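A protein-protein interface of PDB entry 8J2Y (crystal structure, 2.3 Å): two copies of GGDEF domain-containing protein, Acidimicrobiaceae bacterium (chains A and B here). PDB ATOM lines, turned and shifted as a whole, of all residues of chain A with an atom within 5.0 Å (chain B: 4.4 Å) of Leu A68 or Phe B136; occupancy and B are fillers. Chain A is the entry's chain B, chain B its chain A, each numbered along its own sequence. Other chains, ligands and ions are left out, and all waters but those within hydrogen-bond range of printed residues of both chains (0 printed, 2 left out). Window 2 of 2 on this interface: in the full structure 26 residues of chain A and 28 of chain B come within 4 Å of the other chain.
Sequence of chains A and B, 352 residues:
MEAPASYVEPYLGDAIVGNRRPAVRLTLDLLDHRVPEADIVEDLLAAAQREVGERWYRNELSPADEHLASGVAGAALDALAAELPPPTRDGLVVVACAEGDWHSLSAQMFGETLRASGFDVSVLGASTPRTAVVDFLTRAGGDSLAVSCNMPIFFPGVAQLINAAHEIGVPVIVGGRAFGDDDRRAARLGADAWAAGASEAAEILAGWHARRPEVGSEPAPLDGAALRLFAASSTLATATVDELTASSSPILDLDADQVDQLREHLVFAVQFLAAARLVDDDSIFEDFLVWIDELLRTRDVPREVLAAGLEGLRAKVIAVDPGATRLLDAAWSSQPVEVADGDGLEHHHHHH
OD1 of Asp A65 lies within salt-bridge range of NH2 of Arg B139 (3.0 Å).
The backbone carbonyl oxygen of Leu B124 sits at hydrogen-bond distance from a ring nitrogen (ND1) of His A67.
OE1 of Glu A66 lies close to NE2 of His A67 (3.3 Å).
Among the printed residues, merely in contact across the chains: Leu A68 with Phe B136 (3.6 Å), Ala A64 with Ala B132 (3.7 Å), Leu A68 with Val B123 (3.7 Å), Ala A64 with Leu B124 (3.9 Å) and Leu A68 with Leu B124 (3.9 Å).
Of the printed residues of chain B, Ala A64 touches Leu B124 and Ala B132.
Leu A68 touches just these residues of chain B: Val B123, Leu B124 and Phe B136.
Of the printed residues of chain A, Val B123 touches Leu A68 (3.7 Å).
Of the printed residues of chain A, Phe B136 touches Leu A68 (3.6 Å).
The nearest residue of chain B that does not touch Leu A68 is Ser B122 (4.3 Å).
The nearest printed residue of chain A that does not touch Leu B124 is Asp A65 (5.6 Å).
Of the 13 printed residues of chain A, 4 touch a printed residue of chain B.
Hydrophobic or aromatic side chains of chain A that line the printed part of chain B: Ala A64, His A67 and Leu A68.
No position is printed for both chains.
Of the 7 pairs that touch across the chains among the printed residues, none has its exchanged pair printed and touching as well.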
ATOM      1  N   ALA A  15      -9.721  25.071   6.739  1.00  0.00           N
ATOM      2  CA  ALA A  15      -8.761  24.554   7.702  1.00  0.00           C
ATOM      3  C   ALA A  15      -7.327  24.496   7.172  1.00  0.00           C
ATOM      4  O   ALA A  15      -6.392  24.726   7.925  1.00  0.00           O
ATOM      5  CB  ALA A  15      -9.169  23.170   8.199  1.00  0.00           C
ATOM      6  N   ILE A  16      -7.190  24.147   5.888  1.00  0.00           N
ATOM      7  CA  ILE A  16      -5.902  23.963   5.248  1.00  0.00           C
ATOM      8  C   ILE A  16      -5.115  25.271   5.115  1.00  0.00           C
ATOM      9  O   ILE A  16      -3.887  25.248   5.078  1.00  0.00           O
ATOM     10  CB  ILE A  16      -6.155  23.278   3.866  1.00  0.00           C
ATOM     11  CG1 ILE A  16      -6.264  21.774   4.021  1.00  0.00           C
ATOM     12  CG2 ILE A  16      -5.058  23.627   2.805  1.00  0.00           C
ATOM     13  CD1 ILE A  16      -6.921  21.060   2.858  1.00  0.00           C
ATOM     14  N   VAL A  17      -5.823  26.406   5.029  1.00  0.00           N
ATOM     15  CA  VAL A  17      -5.184  27.710   5.063  1.00  0.00           C
ATOM     16  C   VAL A  17      -5.225  28.381   6.440  1.00  0.00           C
ATOM     17  O   VAL A  17      -5.001  29.589   6.516  1.00  0.00           O
ATOM     18  CB  VAL A  17      -5.768  28.682   3.972  1.00  0.00           C
ATOM     19  CG1 VAL A  17      -5.506  28.140   2.570  1.00  0.00           C
ATOM     20  CG2 VAL A  17      -7.254  28.990   4.221  1.00  0.00           C
ATOM     21  N   GLY A  18      -5.526  27.627   7.512  1.00  0.00           N
ATOM     22  CA  GLY A  18      -5.560  28.162   8.867  1.00  0.00           C
ATOM     23  C   GLY A  18      -6.681  29.156   9.186  1.00  0.00           C
ATOM     24  O   GLY A  18      -6.614  29.880  10.174  1.00  0.00           O
ATOM     25  N   ALA A  64       3.323  22.180   6.055  1.00  0.00           N
ATOM     26  CA  ALA A  64       2.974  23.540   6.427  1.00  0.00           C
ATOM     27  C   ALA A  64       1.453  23.651   6.366  1.00  0.00           C
ATOM     28  O   ALA A  64       0.814  24.153   7.289  1.00  0.00           O
ATOM     29  CB  ALA A  64       3.683  24.559   5.520  1.00  0.00           C
ATOM     30  N   ASP A  65       0.880  23.140   5.283  1.00  0.00           N
ATOM     31  CA  ASP A  65      -0.576  23.040   5.163  1.00  0.00           C
ATOM     32  C   ASP A  65      -1.212  22.216   6.275  1.00  0.00           C
ATOM     33  O   ASP A  65      -2.143  22.644   6.952  1.00  0.00           O
ATOM     34  CB  ASP A  65      -0.877  22.427   3.852  1.00  0.00           C
ATOM     35  CG  ASP A  65      -0.286  23.186   2.691  1.00  0.00           C
ATOM     36  OD1 ASP A  65      -0.455  24.444   2.651  1.00  0.00           O
ATOM     37  OD2 ASP A  65       0.288  22.535   1.803  1.00  0.00           O
ATOM     38  N   GLU A  66      -0.684  21.022   6.498  1.00  0.00           N
ATOM     39  CA  GLU A  66      -1.183  20.202   7.589  1.00  0.00           C
ATOM     40  C   GLU A  66      -1.101  20.884   8.959  1.00  0.00           C
ATOM     41  O   GLU A  66      -2.079  20.848   9.718  1.00  0.00           O
ATOM     42  CB  GLU A  66      -0.431  18.874   7.601  1.00  0.00           C
ATOM     43  CG  GLU A  66      -0.621  18.092   8.906  1.00  0.00           C
ATOM     44  CD  GLU A  66       0.389  18.442   9.979  1.00  0.00           C
ATOM     45  OE1 GLU A  66       1.592  18.293   9.674  1.00  0.00           O
ATOM     46  OE2 GLU A  66       0.004  18.953  11.060  1.00  0.00           O
ATOM     47  N   HIS A  67       0.049  21.533   9.272  1.00  0.00           N
ATOM     48  CA  HIS A  67       0.177  22.262  10.526  1.00  0.00           C
ATOM     49  C   HIS A  67      -0.998  23.217  10.714  1.00  0.00           C
ATOM     50  O   HIS A  67      -1.585  23.302  11.779  1.00  0.00           O
ATOM     51  CB  HIS A  67       1.548  22.969  10.650  1.00  0.00           C
ATOM     52  CG  HIS A  67       2.695  22.028  10.866  1.00  0.00           C
ATOM     53  ND1 HIS A  67       3.928  22.336  11.409  1.00  0.00           N
ATOM     54  CD2 HIS A  67       2.788  20.745  10.532  1.00  0.00           C
ATOM     55  CE1 HIS A  67       4.696  21.247  11.419  1.00  0.00           C
ATOM     56  NE2 HIS A  67       3.998  20.251  10.922  1.00  0.00           N
ATOM     57  N   LEU A  68      -1.328  23.983   9.678  1.00  0.00           N
ATOM     58  CA  LEU A  68      -2.493  24.853   9.745  1.00  0.00           C
ATOM     59  C   LEU A  68      -3.788  24.037   9.923  1.00  0.00           C
ATOM     60  O   LEU A  68      -4.591  24.304  10.826  1.00  0.00           O
ATOM     61  CB  LEU A  68      -2.541  25.697   8.480  1.00  0.00           C
ATOM     62  CG  LEU A  68      -1.424  26.789   8.316  1.00  0.00           C
ATOM     63  CD1 LEU A  68      -1.556  27.489   7.025  1.00  0.00           C
ATOM     64  CD2 LEU A  68      -1.525  27.809   9.354  1.00  0.00           C
ATOM     65  N   ALA A  69      -3.983  22.990   9.127  1.00  0.00           N
ATOM     66  CA  ALA A  69      -5.189  22.169   9.312  1.00  0.00           C
ATOM     67  C   ALA A  69      -5.284  21.649  10.750  1.00  0.00           C
ATOM     68  O   ALA A  69      -6.331  21.776  11.366  1.00  0.00           O
ATOM     69  CB  ALA A  69      -5.227  21.028   8.331  1.00  0.00           C
ATOM     70  N   SER A  70      -4.160  21.200  11.328  1.00  0.00           N
ATOM     71  CA  SER A  70      -4.170  20.623  12.669  1.00  0.00           C
ATOM     72  C   SER A  70      -4.455  21.690  13.716  1.00  0.00           C
ATOM     73  O   SER A  70      -5.052  21.432  14.735  1.00  0.00           O
ATOM     74  CB  SER A  70      -2.864  19.890  13.012  1.00  0.00           C
ATOM     75  OG  SER A  70      -2.587  18.756  12.201  1.00  0.00           O
ATOM     76  N   GLY A  71      -4.022  22.918  13.494  1.00  0.00           N
ATOM     77  CA  GLY A  71      -4.380  23.993  14.411  1.00  0.00           C
ATOM     78  C   GLY A  71      -5.888  24.263  14.402  1.00  0.00           C
ATOM     79  O   GLY A  71      -6.492  24.520  15.437  1.00  0.00           O
ATOM     80  N   VAL A  72      -6.492  24.244  13.217  1.00  0.00           N
ATOM     81  CA  VAL A  72      -7.922  24.516  13.113  1.00  0.00           C
ATOM     82  C   VAL A  72      -8.739  23.422  13.824  1.00  0.00           C
ATOM     83  O   VAL A  72      -9.730  23.697  14.505  1.00  0.00           O
ATOM     84  CB  VAL A  72      -8.337  24.730  11.639  1.00  0.00           C
ATOM     85  CG1 VAL A  72      -9.879  24.872  11.512  1.00  0.00           C
ATOM     86  CG2 VAL A  72      -7.609  25.943  11.035  1.00  0.00           C
ATOM     87  N   VAL B  94       4.168  35.046   8.170  1.00  0.00           N
ATOM     88  CA  VAL B  94       4.238  33.618   8.423  1.00  0.00           C
ATOM     89  C   VAL B  94       5.139  33.428   9.636  1.00  0.00           C
ATOM     90  O   VAL B  94       6.314  33.832   9.614  1.00  0.00           O
ATOM     91  CB  VAL B  94       4.813  32.956   7.166  1.00  0.00           C
ATOM     92  CG1 VAL B  94       5.103  31.480   7.383  1.00  0.00           C
ATOM     93  CG2 VAL B  94       3.907  33.225   5.961  1.00  0.00           C
ATOM     94  N   SER B 122      -0.264  33.767   9.613  1.00  0.00           N
ATOM     95  CA  SER B 122      -0.413  32.318   9.597  1.00  0.00           C
ATOM     96  C   SER B 122       0.666  31.691  10.475  1.00  0.00           C
ATOM     97  O   SER B 122       1.853  31.811  10.173  1.00  0.00           O
ATOM     98  CB  SER B 122      -0.323  31.775   8.175  1.00  0.00           C
ATOM     99  OG  SER B 122      -1.441  32.162   7.372  1.00  0.00           O
ATOM    100  N   VAL B 123       0.254  31.052  11.570  1.00  0.00           N
ATOM    101  CA  VAL B 123       1.178  30.429  12.496  1.00  0.00           C
ATOM    102  C   VAL B 123       1.376  28.953  12.189  1.00  0.00           C
ATOM    103  O   VAL B 123       0.500  28.154  12.463  1.00  0.00           O
ATOM    104  CB  VAL B 123       0.705  30.639  13.935  1.00  0.00           C
ATOM    105  CG1 VAL B 123       1.738  30.055  14.949  1.00  0.00           C
ATOM    106  CG2 VAL B 123       0.440  32.126  14.228  1.00  0.00           C
ATOM    107  N   LEU B 124       2.511  28.592  11.593  1.00  0.00           N
ATOM    108  CA  LEU B 124       2.866  27.205  11.361  1.00  0.00           C
ATOM    109  C   LEU B 124       3.215  26.487  12.649  1.00  0.00           C
ATOM    110  O   LEU B 124       3.101  25.270  12.705  1.00  0.00           O
ATOM    111  CB  LEU B 124       4.046  27.070  10.440  1.00  0.00           C
ATOM    112  CG  LEU B 124       3.879  27.733   9.097  1.00  0.00           C
ATOM    113  CD1 LEU B 124       4.945  27.240   8.127  1.00  0.00           C
ATOM    114  CD2 LEU B 124       2.432  27.488   8.505  1.00  0.00           C
ATOM    115  N   ALA B 132       9.404  23.253   2.925  1.00  0.00           N
ATOM    116  CA  ALA B 132       7.950  23.376   3.034  1.00  0.00           C
ATOM    117  C   ALA B 132       7.517  24.770   3.503  1.00  0.00           C
ATOM    118  O   ALA B 132       6.426  25.244   3.172  1.00  0.00           O
ATOM    119  CB  ALA B 132       7.407  22.324   3.995  1.00  0.00           C
ATOM    120  N   VAL B 133       8.380  25.404   4.311  1.00  0.00           N
ATOM    121  CA  VAL B 133       8.135  26.750   4.799  1.00  0.00           C
ATOM    122  C   VAL B 133       8.265  27.756   3.654  1.00  0.00           C
ATOM    123  O   VAL B 133       7.465  28.679   3.530  1.00  0.00           O
ATOM    124  CB  VAL B 133       9.071  27.103   5.981  1.00  0.00           C
ATOM    125  CG1 VAL B 133       8.860  28.539   6.418  1.00  0.00           C
ATOM    126  CG2 VAL B 133       8.854  26.167   7.177  1.00  0.00           C
ATOM    127  N   VAL B 134       9.295  27.566   2.825  1.00  0.00           N
ATOM    128  CA  VAL B 134       9.588  28.483   1.739  1.00  0.00           C
ATOM    129  C   VAL B 134       8.499  28.331   0.681  1.00  0.00           C
ATOM    130  O   VAL B 134       7.961  29.323   0.195  1.00  0.00           O
ATOM    131  CB  VAL B 134      11.049  28.233   1.220  1.00  0.00           C
ATOM    132  CG1 VAL B 134      11.299  28.824  -0.169  1.00  0.00           C
ATOM    133  CG2 VAL B 134      12.069  28.737   2.232  1.00  0.00           C
ATOM    134  N   ASP B 135       8.152  27.082   0.370  1.00  0.00           N
ATOM    135  CA  ASP B 135       7.079  26.816  -0.578  1.00  0.00           C
ATOM    136  C   ASP B 135       5.740  27.403  -0.128  1.00  0.00           C
ATOM    137  O   ASP B 135       5.015  27.942  -0.956  1.00  0.00           O
ATOM    138  CB  ASP B 135       7.011  25.325  -0.896  1.00  0.00           C
ATOM    139  CG  ASP B 135       8.136  24.923  -1.849  1.00  0.00           C
ATOM    140  OD1 ASP B 135       9.198  25.683  -1.924  1.00  0.00           O
ATOM    141  OD2 ASP B 135       7.975  23.909  -2.547  1.00  0.00           O
ATOM    142  N   PHE B 136       5.433  27.343   1.178  1.00  0.00           N
ATOM    143  CA  PHE B 136       4.294  28.072   1.731  1.00  0.00           C
ATOM    144  C   PHE B 136       4.350  29.594   1.539  1.00  0.00           C
ATOM    145  O   PHE B 136       3.344  30.220   1.179  1.00  0.00           O
ATOM    146  CB  PHE B 136       4.199  27.809   3.215  1.00  0.00           C
ATOM    147  CG  PHE B 136       2.981  28.418   3.836  1.00  0.00           C
ATOM    148  CD1 PHE B 136       1.752  27.779   3.751  1.00  0.00           C
ATOM    149  CD2 PHE B 136       3.054  29.617   4.524  1.00  0.00           C
ATOM    150  CE1 PHE B 136       0.616  28.337   4.330  1.00  0.00           C
ATOM    151  CE2 PHE B 136       1.931  30.183   5.086  1.00  0.00           C
ATOM    152  CZ  PHE B 136       0.699  29.530   4.987  1.00  0.00           C
ATOM    153  N   LEU B 137       5.538  30.184   1.810  1.00  0.00           N
ATOM    154  CA  LEU B 137       5.752  31.617   1.630  1.00  0.00           C
ATOM    155  C   LEU B 137       5.444  31.987   0.199  1.00  0.00           C
ATOM    156  O   LEU B 137       4.718  32.944  -0.019  1.00  0.00           O
ATOM    157  CB  LEU B 137       7.204  32.065   1.950  1.00  0.00           C
ATOM    158  CG  LEU B 137       7.487  32.162   3.428  1.00  0.00           C
ATOM    159  CD1 LEU B 137       8.927  32.201   3.667  1.00  0.00           C
ATOM    160  CD2 LEU B 137       6.756  33.366   4.022  1.00  0.00           C
ATOM    161  N   THR B 138       5.996  31.197  -0.734  1.00  0.00           N
ATOM    162  CA  THR B 138       5.761  31.384  -2.157  1.00  0.00           C
ATOM    163  C   THR B 138       4.292  31.294  -2.569  1.00  0.00           C
ATOM    164  O   THR B 138       3.810  32.146  -3.310  1.00  0.00           O
ATOM    165  CB  THR B 138       6.501  30.311  -2.989  1.00  0.00           C
ATOM    166  OG1 THR B 138       7.899  30.385  -2.761  1.00  0.00           O
ATOM    167  CG2 THR B 138       6.226  30.450  -4.509  1.00  0.00           C
ATOM    168  N   ARG B 139       3.602  30.240  -2.106  1.00  0.00           N
ATOM    169  CA  ARG B 139       2.234  29.960  -2.538  1.00  0.00           C
ATOM    170  C   ARG B 139       1.234  30.909  -1.882  1.00  0.00           C
ATOM    171  O   ARG B 139       0.296  31.375  -2.524  1.00  0.00           O
ATOM    172  CB  ARG B 139       1.847  28.502  -2.234  1.00  0.00           C
ATOM    173  CG  ARG B 139       2.499  27.405  -3.129  1.00  0.00           C
ATOM    174  CD  ARG B 139       1.985  25.977  -2.750  1.00  0.00           C
ATOM    175  NE  ARG B 139       2.274  25.621  -1.350  1.00  0.00           N
ATOM    176  CZ  ARG B 139       1.364  25.527  -0.372  1.00  0.00           C
ATOM    177  NH1 ARG B 139       0.065  25.604  -0.630  1.00  0.00           N
ATOM    178  NH2 ARG B 139       1.774  25.388   0.894  1.00  0.00           N
ATOM    179  N   ALA B 140       1.478  31.238  -0.611  1.00  0.00           N
ATOM    180  CA  ALA B 140       0.623  32.139   0.144  1.00  0.00           C
ATOM    181  C   ALA B 140       0.914  33.627  -0.063  1.00  0.00           C
ATOM    182  O   ALA B 140       0.196  34.457   0.494  1.00  0.00           O
ATOM    183  CB  ALA B 140       0.746  31.810   1.623  1.00  0.00           C
